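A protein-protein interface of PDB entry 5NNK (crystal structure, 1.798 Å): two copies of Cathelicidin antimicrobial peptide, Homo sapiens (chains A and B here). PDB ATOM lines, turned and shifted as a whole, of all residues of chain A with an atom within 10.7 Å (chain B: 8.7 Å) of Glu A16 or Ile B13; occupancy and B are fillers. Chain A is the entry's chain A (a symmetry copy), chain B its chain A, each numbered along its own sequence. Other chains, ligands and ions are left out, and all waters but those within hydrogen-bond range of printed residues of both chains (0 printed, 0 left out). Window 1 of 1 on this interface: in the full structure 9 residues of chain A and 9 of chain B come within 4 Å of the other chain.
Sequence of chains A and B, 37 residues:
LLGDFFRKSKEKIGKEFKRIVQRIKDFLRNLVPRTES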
ATOM      1  N   LYS A   8     -17.212   4.401  -7.154  1.00  0.00           N
ATOM      2  CA  LYS A   8     -17.262   5.796  -6.724  1.00  0.00           C
ATOM      3  C   LYS A   8     -15.947   6.514  -7.032  1.00  0.00           C
ATOM      4  O   LYS A   8     -15.931   7.556  -7.706  1.00  0.00           O
ATOM      5  CB  LYS A   8     -17.599   5.853  -5.226  1.00  0.00           C
ATOM      6  CG  LYS A   8     -17.990   7.241  -4.703  1.00  0.00           C
ATOM      7  CD  LYS A   8     -19.250   7.218  -3.810  1.00  0.00           C
ATOM      8  CE  LYS A   8     -18.939   6.992  -2.326  1.00  0.00           C
ATOM      9  NZ  LYS A   8     -20.167   7.080  -1.470  1.00  0.00           N
ATOM     10  N   SER A   9     -14.827   5.965  -6.556  1.00  0.00           N
ATOM     11  CA  SER A   9     -13.528   6.569  -6.836  1.00  0.00           C
ATOM     12  C   SER A   9     -13.295   6.714  -8.332  1.00  0.00           C
ATOM     13  O   SER A   9     -12.893   7.780  -8.807  1.00  0.00           O
ATOM     14  CB  SER A   9     -12.410   5.734  -6.215  1.00  0.00           C
ATOM     15  OG  SER A   9     -12.273   6.001  -4.833  1.00  0.00           O
ATOM     16  N   LYS A  10     -13.519   5.640  -9.093  1.00  0.00           N
ATOM     17  CA  LYS A  10     -13.263   5.701 -10.529  1.00  0.00           C
ATOM     18  C   LYS A  10     -14.098   6.788 -11.194  1.00  0.00           C
ATOM     19  O   LYS A  10     -13.621   7.466 -12.113  1.00  0.00           O
ATOM     20  CB  LYS A  10     -13.536   4.339 -11.177  1.00  0.00           C
ATOM     21  CG  LYS A  10     -12.418   3.310 -10.989  1.00  0.00           C
ATOM     22  CD  LYS A  10     -12.909   1.867 -11.183  1.00  0.00           C
ATOM     23  CE  LYS A  10     -13.605   1.639 -12.527  1.00  0.00           C
ATOM     24  NZ  LYS A  10     -14.488   0.433 -12.515  1.00  0.00           N
ATOM     25  N   GLU A  11     -15.332   6.991 -10.730  1.00  0.00           N
ATOM     26  CA  GLU A  11     -16.168   8.033 -11.317  1.00  0.00           C
ATOM     27  C   GLU A  11     -15.657   9.424 -10.963  1.00  0.00           C
ATOM     28  O   GLU A  11     -15.635  10.317 -11.820  1.00  0.00           O
ATOM     29  CB  GLU A  11     -17.617   7.854 -10.875  1.00  0.00           C
ATOM     30  CG  GLU A  11     -18.452   7.085 -11.891  1.00  0.00           C
ATOM     31  CD  GLU A  11     -19.851   6.781 -11.396  1.00  0.00           C
ATOM     32  OE1 GLU A  11     -20.346   7.529 -10.526  1.00  0.00           O
ATOM     33  OE2 GLU A  11     -20.454   5.795 -11.876  1.00  0.00           O
ATOM     34  N   LYS A  12     -15.237   9.635  -9.712  1.00  0.00           N
ATOM     35  CA  LYS A  12     -14.645  10.924  -9.357  1.00  0.00           C
ATOM     36  C   LYS A  12     -13.407  11.214 -10.211  1.00  0.00           C
ATOM     37  O   LYS A  12     -13.298  12.282 -10.835  1.00  0.00           O
ATOM     38  CB  LYS A  12     -14.316  10.951  -7.860  1.00  0.00           C
ATOM     39  CG  LYS A  12     -15.565  10.857  -6.959  1.00  0.00           C
ATOM     40  CD  LYS A  12     -15.246  10.745  -5.468  1.00  0.00           C
ATOM     41  CE  LYS A  12     -16.534  10.741  -4.642  1.00  0.00           C
ATOM     42  NZ  LYS A  12     -16.316  10.836  -3.165  1.00  0.00           N
ATOM     43  N   ILE A  13     -12.475  10.253 -10.278  1.00  0.00           N
ATOM     44  CA  ILE A  13     -11.271  10.427 -11.096  1.00  0.00           C
ATOM     45  C   ILE A  13     -11.647  10.787 -12.528  1.00  0.00           C
ATOM     46  O   ILE A  13     -11.094  11.724 -13.120  1.00  0.00           O
ATOM     47  CB  ILE A  13     -10.395   9.158 -11.047  1.00  0.00           C
ATOM     48  CG1 ILE A  13      -9.777   8.974  -9.653  1.00  0.00           C
ATOM     49  CG2 ILE A  13      -9.286   9.224 -12.115  1.00  0.00           C
ATOM     50  CD1 ILE A  13      -9.002   7.659  -9.471  1.00  0.00           C
ATOM     51  N   GLY A  14     -12.583  10.035 -13.116  1.00  0.00           N
ATOM     52  CA  GLY A  14     -12.997  10.335 -14.478  1.00  0.00           C
ATOM     53  C   GLY A  14     -13.545  11.747 -14.615  1.00  0.00           C
ATOM     54  O   GLY A  14     -13.240  12.452 -15.582  1.00  0.00           O
ATOM     55  N   LYS A  15     -14.359  12.171 -13.648  1.00  0.00           N
ATOM     56  CA  LYS A  15     -14.858  13.542 -13.621  1.00  0.00           C
ATOM     57  C   LYS A  15     -13.715  14.543 -13.753  1.00  0.00           C
ATOM     58  O   LYS A  15     -13.675  15.352 -14.691  1.00  0.00           O
ATOM     59  CB  LYS A  15     -15.634  13.766 -12.317  1.00  0.00           C
ATOM     60  CG  LYS A  15     -16.423  15.076 -12.206  1.00  0.00           C
ATOM     61  CD  LYS A  15     -17.366  15.008 -10.994  1.00  0.00           C
ATOM     62  CE  LYS A  15     -17.937  16.367 -10.574  1.00  0.00           C
ATOM     63  NZ  LYS A  15     -19.088  16.837 -11.408  1.00  0.00           N
ATOM     64  N   GLU A  16     -12.763  14.492 -12.814  1.00  0.00           N
ATOM     65  CA  GLU A  16     -11.679  15.474 -12.813  1.00  0.00           C
ATOM     66  C   GLU A  16     -10.876  15.419 -14.107  1.00  0.00           C
ATOM     67  O   GLU A  16     -10.524  16.458 -14.680  1.00  0.00           O
ATOM     68  CB  GLU A  16     -10.772  15.249 -11.603  1.00  0.00           C
ATOM     69  CG  GLU A  16     -11.478  15.489 -10.286  1.00  0.00           C
ATOM     70  CD  GLU A  16     -12.087  16.879 -10.200  1.00  0.00           C
ATOM     71  OE1 GLU A  16     -11.527  17.811 -10.817  1.00  0.00           O
ATOM     72  OE2 GLU A  16     -13.131  17.037  -9.530  1.00  0.00           O
ATOM     73  N   PHE A  17     -10.567  14.215 -14.587  1.00  0.00           N
ATOM     74  CA  PHE A  17      -9.805  14.110 -15.822  1.00  0.00           C
ATOM     75  C   PHE A  17     -10.538  14.778 -16.977  1.00  0.00           C
ATOM     76  O   PHE A  17      -9.921  15.466 -17.796  1.00  0.00           O
ATOM     77  CB  PHE A  17      -9.523  12.651 -16.154  1.00  0.00           C
ATOM     78  CG  PHE A  17      -8.577  12.472 -17.303  1.00  0.00           C
ATOM     79  CD1 PHE A  17      -7.225  12.731 -17.136  1.00  0.00           C
ATOM     80  CD2 PHE A  17      -9.029  12.050 -18.548  1.00  0.00           C
ATOM     81  CE1 PHE A  17      -6.334  12.570 -18.186  1.00  0.00           C
ATOM     82  CE2 PHE A  17      -8.143  11.885 -19.607  1.00  0.00           C
ATOM     83  CZ  PHE A  17      -6.793  12.145 -19.422  1.00  0.00           C
ATOM     84  N   LYS A  18     -11.857  14.584 -17.064  1.00  0.00           N
ATOM     85  CA  LYS A  18     -12.608  15.233 -18.136  1.00  0.00           C
ATOM     86  C   LYS A  18     -12.566  16.747 -17.988  1.00  0.00           C
ATOM     87  O   LYS A  18     -12.434  17.474 -18.982  1.00  0.00           O
ATOM     88  CB  LYS A  18     -14.049  14.720 -18.158  1.00  0.00           C
ATOM     89  CG  LYS A  18     -14.194  13.428 -18.952  1.00  0.00           C
ATOM     90  CD  LYS A  18     -15.197  12.466 -18.333  1.00  0.00           C
ATOM     91  CE  LYS A  18     -14.929  11.035 -18.792  1.00  0.00           C
ATOM     92  NZ  LYS A  18     -16.011  10.078 -18.418  1.00  0.00           N
ATOM     93  N   ARG A  19     -12.659  17.244 -16.753  1.00  0.00           N
ATOM     94  CA  ARG A  19     -12.500  18.676 -16.515  1.00  0.00           C
ATOM     95  C   ARG A  19     -11.168  19.180 -17.074  1.00  0.00           C
ATOM     96  O   ARG A  19     -11.121  20.154 -17.839  1.00  0.00           O
ATOM     97  CB  ARG A  19     -12.603  18.947 -15.011  1.00  0.00           C
ATOM     98  CG  ARG A  19     -12.830  20.392 -14.622  1.00  0.00           C
ATOM     99  CD  ARG A  19     -13.518  20.464 -13.264  1.00  0.00           C
ATOM    100  NE  ARG A  19     -14.910  20.032 -13.366  1.00  0.00           N
ATOM    101  CZ  ARG A  19     -15.650  19.604 -12.348  1.00  0.00           C
ATOM    102  NH1 ARG A  19     -15.143  19.533 -11.124  1.00  0.00           N
ATOM    103  NH2 ARG A  19     -16.906  19.237 -12.560  1.00  0.00           N
ATOM    104  N   ILE A  20     -10.073  18.512 -16.699  1.00  0.00           N
ATOM    105  CA  ILE A  20      -8.743  18.909 -17.165  1.00  0.00           C
ATOM    106  C   ILE A  20      -8.692  18.921 -18.690  1.00  0.00           C
ATOM    107  O   ILE A  20      -8.317  19.925 -19.311  1.00  0.00           O
ATOM    108  CB  ILE A  20      -7.672  17.969 -16.580  1.00  0.00           C
ATOM    109  CG1 ILE A  20      -7.623  18.094 -15.054  1.00  0.00           C
ATOM    110  CG2 ILE A  20      -6.297  18.257 -17.197  1.00  0.00           C
ATOM    111  CD1 ILE A  20      -6.730  17.066 -14.386  1.00  0.00           C
ATOM    112  N   VAL A  21      -9.048  17.796 -19.316  1.00  0.00           N
ATOM    113  CA  VAL A  21      -8.979  17.704 -20.775  1.00  0.00           C
ATOM    114  C   VAL A  21      -9.780  18.828 -21.416  1.00  0.00           C
ATOM    115  O   VAL A  21      -9.352  19.422 -22.414  1.00  0.00           O
ATOM    116  CB  VAL A  21      -9.466  16.320 -21.248  1.00  0.00           C
ATOM    117  CG1 VAL A  21      -9.641  16.281 -22.768  1.00  0.00           C
ATOM    118  CG2 VAL A  21      -8.489  15.233 -20.816  1.00  0.00           C
ATOM    119  N   GLN A  22     -10.953  19.138 -20.862  1.00  0.00           N
ATOM    120  CA  GLN A  22     -11.769  20.204 -21.430  1.00  0.00           C
ATOM    121  C   GLN A  22     -11.055  21.546 -21.353  1.00  0.00           C
ATOM    122  O   GLN A  22     -11.061  22.317 -22.321  1.00  0.00           O
ATOM    123  CB  GLN A  22     -13.117  20.273 -20.713  1.00  0.00           C
ATOM    124  CG  GLN A  22     -14.113  21.243 -21.348  1.00  0.00           C
ATOM    125  CD  GLN A  22     -14.508  20.847 -22.765  1.00  0.00           C
ATOM    126  OE1 GLN A  22     -14.950  19.723 -23.009  1.00  0.00           O
ATOM    127  NE2 GLN A  22     -14.345  21.773 -23.708  1.00  0.00           N
ATOM    128  N   ARG A  23     -10.434  21.850 -20.208  1.00  0.00           N
ATOM    129  CA  ARG A  23      -9.746  23.134 -20.080  1.00  0.00           C
ATOM    130  C   ARG A  23      -8.523  23.214 -20.990  1.00  0.00           C
ATOM    131  O   ARG A  23      -8.228  24.283 -21.549  1.00  0.00           O
ATOM    132  CB  ARG A  23      -9.368  23.370 -18.617  1.00  0.00           C
ATOM    133  CG  ARG A  23     -10.535  23.923 -17.797  1.00  0.00           C
ATOM    134  CD  ARG A  23     -10.620  23.336 -16.390  1.00  0.00           C
ATOM    135  NE  ARG A  23      -9.770  24.050 -15.438  1.00  0.00           N
ATOM    136  CZ  ARG A  23      -9.654  23.728 -14.152  1.00  0.00           C
ATOM    137  NH1 ARG A  23     -10.330  22.700 -13.655  1.00  0.00           N
ATOM    138  NH2 ARG A  23      -8.859  24.434 -13.357  1.00  0.00           N
ATOM    139  N   ILE A  24      -7.812  22.100 -21.170  1.00  0.00           N
ATOM    140  CA  ILE A  24      -6.693  22.075 -22.108  1.00  0.00           C
ATOM    141  C   ILE A  24      -7.190  22.278 -23.534  1.00  0.00           C
ATOM    142  O   ILE A  24      -6.562  22.985 -24.333  1.00  0.00           O
ATOM    143  CB  ILE A  24      -5.912  20.757 -21.948  1.00  0.00           C
ATOM    144  CG1 ILE A  24      -5.190  20.760 -20.596  1.00  0.00           C
ATOM    145  CG2 ILE A  24      -4.927  20.561 -23.098  1.00  0.00           C
ATOM    146  CD1 ILE A  24      -4.562  19.441 -20.204  1.00  0.00           C
ATOM    147  N   LEU B   2       1.123  18.329 -14.638  1.00  0.00           N
ATOM    148  CA  LEU B   2       1.090  19.446 -15.592  1.00  0.00           C
ATOM    149  C   LEU B   2       1.598  20.734 -14.938  1.00  0.00           C
ATOM    150  O   LEU B   2       0.901  21.741 -14.841  1.00  0.00           O
ATOM    151  CB  LEU B   2      -0.314  19.649 -16.150  1.00  0.00           C
ATOM    152  CG  LEU B   2      -1.051  18.403 -16.631  1.00  0.00           C
ATOM    153  CD1 LEU B   2      -1.995  17.882 -15.548  1.00  0.00           C
ATOM    154  CD2 LEU B   2      -1.780  18.602 -17.948  1.00  0.00           C
ATOM    155  N   PHE B   6      -3.894  23.058 -12.477  1.00  0.00           N
ATOM    156  CA  PHE B   6      -4.861  22.048 -12.050  1.00  0.00           C
ATOM    157  C   PHE B   6      -4.515  21.496 -10.672  1.00  0.00           C
ATOM    158  O   PHE B   6      -4.648  20.300 -10.421  1.00  0.00           O
ATOM    159  CB  PHE B   6      -4.956  20.914 -13.069  1.00  0.00           C
ATOM    160  CG  PHE B   6      -5.148  21.390 -14.479  1.00  0.00           C
ATOM    161  CD1 PHE B   6      -6.305  22.050 -14.842  1.00  0.00           C
ATOM    162  CD2 PHE B   6      -4.173  21.189 -15.439  1.00  0.00           C
ATOM    163  CE1 PHE B   6      -6.490  22.498 -16.136  1.00  0.00           C
ATOM    164  CE2 PHE B   6      -4.352  21.639 -16.737  1.00  0.00           C
ATOM    165  CZ  PHE B   6      -5.511  22.293 -17.082  1.00  0.00           C
ATOM    166  N   ARG B   7      -4.059  22.373  -9.779  1.00  0.00           N
ATOM    167  CA  ARG B   7      -3.780  21.966  -8.409  1.00  0.00           C
ATOM    168  C   ARG B   7      -4.961  21.201  -7.815  1.00  0.00           C
ATOM    169  O   ARG B   7      -4.805  20.089  -7.292  1.00  0.00           O
ATOM    170  CB  ARG B   7      -3.450  23.206  -7.577  1.00  0.00           C
ATOM    171  CG  ARG B   7      -2.973  22.908  -6.178  1.00  0.00           C
ATOM    172  CD  ARG B   7      -1.457  22.985  -6.094  1.00  0.00           C
ATOM    173  NE  ARG B   7      -0.987  22.775  -4.729  1.00  0.00           N
ATOM    174  CZ  ARG B   7       0.285  22.850  -4.352  1.00  0.00           C
ATOM    175  NH1 ARG B   7       1.235  23.131  -5.233  1.00  0.00           N
ATOM    176  NH2 ARG B   7       0.606  22.641  -3.084  1.00  0.00           N
ATOM    177  N   LYS B   8      -6.163  21.774  -7.918  1.00  0.00           N
ATOM    178  CA  LYS B   8      -7.333  21.203  -7.256  1.00  0.00           C
ATOM    179  C   LYS B   8      -7.669  19.823  -7.825  1.00  0.00           C
ATOM    180  O   LYS B   8      -7.759  18.832  -7.084  1.00  0.00           O
ATOM    181  CB  LYS B   8      -8.516  22.173  -7.391  1.00  0.00           C
ATOM    182  CG  LYS B   8      -9.716  21.859  -6.489  1.00  0.00           C
ATOM    183  CD  LYS B   8     -10.267  23.105  -5.759  1.00  0.00           C
ATOM    184  CE  LYS B   8     -11.345  23.849  -6.557  1.00  0.00           C
ATOM    185  NZ  LYS B   8     -11.936  24.989  -5.783  1.00  0.00           N
ATOM    186  N   SER B   9      -7.846  19.736  -9.145  1.00  0.00           N
ATOM    187  CA  SER B   9      -8.134  18.449  -9.771  1.00  0.00           C
ATOM    188  C   SER B   9      -7.061  17.421  -9.446  1.00  0.00           C
ATOM    189  O   SER B   9      -7.367  16.291  -9.055  1.00  0.00           O
ATOM    190  CB  SER B   9      -8.255  18.611 -11.285  1.00  0.00           C
ATOM    191  OG  SER B   9      -9.527  19.111 -11.650  1.00  0.00           O
ATOM    192  N   LYS B  10      -5.789  17.788  -9.623  1.00  0.00           N
ATOM    193  CA  LYS B  10      -4.716  16.830  -9.379  1.00  0.00           C
ATOM    194  C   LYS B  10      -4.743  16.324  -7.941  1.00  0.00           C
ATOM    195  O   LYS B  10      -4.474  15.142  -7.691  1.00  0.00           O
ATOM    196  CB  LYS B  10      -3.357  17.458  -9.704  1.00  0.00           C
ATOM    197  CG  LYS B  10      -3.018  17.503 -11.197  1.00  0.00           C
ATOM    198  CD  LYS B  10      -1.945  18.553 -11.524  1.00  0.00           C
ATOM    199  CE  LYS B  10      -0.662  18.385 -10.705  1.00  0.00           C
ATOM    200  NZ  LYS B  10       0.150  19.638 -10.655  1.00  0.00           N
ATOM    201  N   GLU B  11      -5.091  17.190  -6.987  1.00  0.00           N
ATOM    202  CA  GLU B  11      -5.152  16.754  -5.597  1.00  0.00           C
ATOM    203  C   GLU B  11      -6.323  15.809  -5.359  1.00  0.00           C
ATOM    204  O   GLU B  11      -6.180  14.805  -4.650  1.00  0.00           O
ATOM    205  CB  GLU B  11      -5.230  17.964  -4.670  1.00  0.00           C
ATOM    206  CG  GLU B  11      -3.868  18.377  -4.127  1.00  0.00           C
ATOM    207  CD  GLU B  11      -3.919  19.660  -3.322  1.00  0.00           C
ATOM    208  OE1 GLU B  11      -5.000  19.977  -2.781  1.00  0.00           O
ATOM    209  OE2 GLU B  11      -2.879  20.352  -3.234  1.00  0.00           O
ATOM    210  N   LYS B  12      -7.490  16.102  -5.941  1.00  0.00           N
ATOM    211  CA  LYS B  12      -8.610  15.170  -5.823  1.00  0.00           C
ATOM    212  C   LYS B  12      -8.248  13.800  -6.402  1.00  0.00           C
ATOM    213  O   LYS B  12      -8.404  12.763  -5.736  1.00  0.00           O
ATOM    214  CB  LYS B  12      -9.852  15.760  -6.502  1.00  0.00           C
ATOM    215  CG  LYS B  12     -10.367  17.045  -5.822  1.00  0.00           C
ATOM    216  CD  LYS B  12     -11.520  17.720  -6.567  1.00  0.00           C
ATOM    217  CE  LYS B  12     -12.025  18.935  -5.786  1.00  0.00           C
ATOM    218  NZ  LYS B  12     -13.279  19.539  -6.336  1.00  0.00           N
ATOM    219  N   ILE B  13      -7.728  13.779  -7.637  1.00  0.00           N
ATOM    220  CA  ILE B  13      -7.321  12.517  -8.262  1.00  0.00           C
ATOM    221  C   ILE B  13      -6.357  11.761  -7.357  1.00  0.00           C
ATOM    222  O   ILE B  13      -6.511  10.554  -7.123  1.00  0.00           O
ATOM    223  CB  ILE B  13      -6.701  12.776  -9.651  1.00  0.00           C
ATOM    224  CG1 ILE B  13      -7.768  13.264 -10.643  1.00  0.00           C
ATOM    225  CG2 ILE B  13      -6.020  11.501 -10.186  1.00  0.00           C
ATOM    226  CD1 ILE B  13      -7.214  13.681 -12.016  1.00  0.00           C
ATOM    227  N   GLY B  14      -5.333  12.453  -6.848  1.00  0.00           N
ATOM    228  CA  GLY B  14      -4.385  11.792  -5.964  1.00  0.00           C
ATOM    229  C   GLY B  14      -5.057  11.205  -4.734  1.00  0.00           C
ATOM    230  O   GLY B  14      -4.747  10.084  -4.317  1.00  0.00           O
ATOM    231  N   LYS B  15      -5.985  11.957  -4.141  1.00  0.00           N
ATOM    232  CA  LYS B  15      -6.769  11.452  -3.018  1.00  0.00           C
ATOM    233  C   LYS B  15      -7.394  10.101  -3.350  1.00  0.00           C
ATOM    234  O   LYS B  15      -7.138   9.092  -2.677  1.00  0.00           O
ATOM    235  CB  LYS B  15      -7.848  12.481  -2.659  1.00  0.00           C
ATOM    236  CG  LYS B  15      -8.629  12.232  -1.363  1.00  0.00           C
ATOM    237  CD  LYS B  15      -9.442  13.485  -1.003  1.00  0.00           C
ATOM    238  CE  LYS B  15     -10.522  13.242   0.057  1.00  0.00           C
ATOM    239  NZ  LYS B  15     -10.010  13.203   1.463  1.00  0.00           N
ATOM    240  N   GLU B  16      -8.217  10.065  -4.404  1.00  0.00           N
ATOM    241  CA  GLU B  16      -8.930   8.832  -4.738  1.00  0.00           C
ATOM    242  C   GLU B  16      -7.962   7.692  -5.030  1.00  0.00           C
ATOM    243  O   GLU B  16      -8.169   6.555  -4.587  1.00  0.00           O
ATOM    244  CB  GLU B  16      -9.858   9.073  -5.928  1.00  0.00           C
ATOM    245  CG  GLU B  16     -10.966  10.057  -5.620  1.00  0.00           C
ATOM    246  CD  GLU B  16     -11.796   9.639  -4.418  1.00  0.00           C
ATOM    247  OE1 GLU B  16     -11.928   8.418  -4.184  1.00  0.00           O
ATOM    248  OE2 GLU B  16     -12.303  10.528  -3.698  1.00  0.00           O
ATOM    249  N   PHE B  17      -6.897   7.968  -5.782  1.00  0.00           N
ATOM    250  CA  PHE B  17      -5.942   6.913  -6.085  1.00  0.00           C
ATOM    251  C   PHE B  17      -5.341   6.334  -4.812  1.00  0.00           C
ATOM    252  O   PHE B  17      -5.173   5.116  -4.696  1.00  0.00           O
ATOM    253  CB  PHE B  17      -4.839   7.436  -6.994  1.00  0.00           C
ATOM    254  CG  PHE B  17      -3.929   6.362  -7.509  1.00  0.00           C
ATOM    255  CD1 PHE B  17      -4.371   5.488  -8.491  1.00  0.00           C
ATOM    256  CD2 PHE B  17      -2.636   6.216  -7.015  1.00  0.00           C
ATOM    257  CE1 PHE B  17      -3.544   4.489  -8.980  1.00  0.00           C
ATOM    258  CE2 PHE B  17      -1.799   5.218  -7.501  1.00  0.00           C
ATOM    259  CZ  PHE B  17      -2.257   4.354  -8.486  1.00  0.00           C
ATOM    260  N   LYS B  18      -5.005   7.192  -3.844  1.00  0.00           N
ATOM    261  CA  LYS B  18      -4.456   6.680  -2.590  1.00  0.00           C
ATOM    262  C   LYS B  18      -5.484   5.832  -1.855  1.00  0.00           C
ATOM    263  O   LYS B  18      -5.146   4.786  -1.283  1.00  0.00           O
ATOM    264  CB  LYS B  18      -3.967   7.835  -1.716  1.00  0.00           C
ATOM    265  CG  LYS B  18      -2.548   8.267  -2.063  1.00  0.00           C
ATOM    266  CD  LYS B  18      -2.349   9.772  -1.962  1.00  0.00           C
ATOM    267  CE  LYS B  18      -1.160  10.219  -2.808  1.00  0.00           C
ATOM    268  NZ  LYS B  18      -0.760  11.637  -2.571  1.00  0.00           N
ATOM    269  N   ARG B  19      -6.750   6.252  -1.872  1.00  0.00           N
ATOM    270  CA  ARG B  19      -7.814   5.431  -1.300  1.00  0.00           C
ATOM    271  C   ARG B  19      -7.825   4.035  -1.925  1.00  0.00           C
ATOM    272  O   ARG B  19      -7.805   3.016  -1.219  1.00  0.00           O
ATOM    273  CB  ARG B  19      -9.156   6.137  -1.509  1.00  0.00           C
ATOM    274  CG  ARG B  19     -10.303   5.620  -0.667  1.00  0.00           C
ATOM    275  CD  ARG B  19     -11.344   6.716  -0.475  1.00  0.00           C
ATOM    276  NE  ARG B  19     -10.847   7.751   0.427  1.00  0.00           N
ATOM    277  CZ  ARG B  19     -11.313   8.995   0.490  1.00  0.00           C
ATOM    278  NH1 ARG B  19     -12.300   9.389  -0.304  1.00  0.00           N
ATOM    279  NH2 ARG B  19     -10.781   9.850   1.352  1.00  0.00           N
ATOM    280  N   ILE B  20      -7.847   3.979  -3.261  1.00  0.00           N
ATOM    281  CA  ILE B  20      -7.867   2.698  -3.968  1.00  0.00           C
ATOM    282  C   ILE B  20      -6.671   1.843  -3.561  1.00  0.00           C
ATOM    283  O   ILE B  20      -6.822   0.687  -3.141  1.00  0.00           O
ATOM    284  CB  ILE B  20      -7.892   2.931  -5.490  1.00  0.00           C
ATOM    285  CG1 ILE B  20      -9.184   3.645  -5.904  1.00  0.00           C
ATOM    286  CG2 ILE B  20      -7.733   1.606  -6.248  1.00  0.00           C
ATOM    287  CD1 ILE B  20      -9.200   4.082  -7.356  1.00  0.00           C
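The side-chain hydroxyl (OG) of Ser B9 lies within hydrogen-bond range of the side-chain carboxylate (OE1) of Glu A16 (2.5 Å). The side-chain carboxylate (OE1) of Glu B16 is in hydrogen-bond range of the side-chain hydroxyl (OG) of Ser A9 (2.5 Å).
OE2 of Glu B16 is in salt-bridge range of NH1 of Arg B19 (3.6 Å). The side-chain carboxylate (OE2) of Glu A16 lies within salt-bridge range of the guanidinium group (NH1) of Arg A19 (3.6 Å).
CD1 of Ile B20 touches CB of Ser A9 (3.8 Å). CD of Lys A12 touches OE2 of Glu B16, 3.4 Å away. Glu B16 touches Ile A13 (CB to CG1, 3.7 Å). Glu A16 touches Lys B12. Glu A16 touches Ile B13. CE2 of Phe B6 touches CG2 of Ile A20 (3.9 Å). Ile A20 touches Ser B9 (CD1 to CB, 3.8 Å). CE1 of Phe B6 touches NE of Arg A23, 3.7 Å away. Leu B2 touches Ile A24. Ile A24 touches Phe B6 (CG1 to CZ, 3.8 Å).
Glu A16 touches just these residues of chain B: Ser B9, Lys B12 and Ile B13. Of chain A, only Glu A16 comes within 4 Å of Ile B13. No residue of chain B comes within 4 Å of Gly A14. Of chain A, only Glu A16 comes within 4 Å of Lys B12. No residue of chain A comes within 4 Å of Gly B14. Printed residues of chain A within 4 Å of Ile B20: Ser A9 (3.8 Å). Of the printed residues of chain A, Leu B2 touches Ile A24 (3.7 Å). Printed residues of chain B within 4 Å of Ile A20: Phe B6 and Ser B9. Of the printed residues of chain A, Phe B6 touches Ile A20 (3.9 Å), Arg A23 (3.7 Å) and Ile A24 (3.8 Å). Printed residues of chain B within 4 Å of Ser A9: Glu B16 and Ile B20. Phe A17 touches none of the printed residues of chain B. Arg A19 touches none of the printed residues of chain B.
Printed residues of chain B that touch a printed residue of chain A: Leu B2, Phe B6, Ser B9, Lys B12, Ile B13, Glu B16 and Ile B20. Hydrophobic or aromatic side chains of chain B that line the printed part of chain A: Leu B2, Phe B6, Ile B13 and Ile B20. Printed residues of chain A that touch a printed residue of chain B: Ser A9, Lys A12, Ile A13, Glu A16, Ile A20, Arg A23 and Ile A24. Hydrophobic or aromatic side chains of chain A within 4 Å of the printed part of chain B: Ile A13, Ile A20 and Ile A24. Along chain A the printed residues that touch a printed residue of chain B span positions 9 to 24. Among the printed residues, no Asp or Glu carboxylate lies within 4 Å of a Lys or Arg side-chain nitrogen of the other chain.
Ser A9 touches Glu B16, and with the chains exchanged Glu A16 touches Ser B9. Ser A9 touches Ile B20, and with the chains exchanged Ile A20 touches Ser B9. Lys A12 touches Glu B16, and with the chains exchanged Glu A16 touches Lys B12. Ile A13 touches Glu B16, and with the chains exchanged Glu A16 touches Ile B13. 13 positions are printed for both chains. Of the 12 pairs that touch across the chains among the printed residues, 8 have their exchanged pair printed and touching as well.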
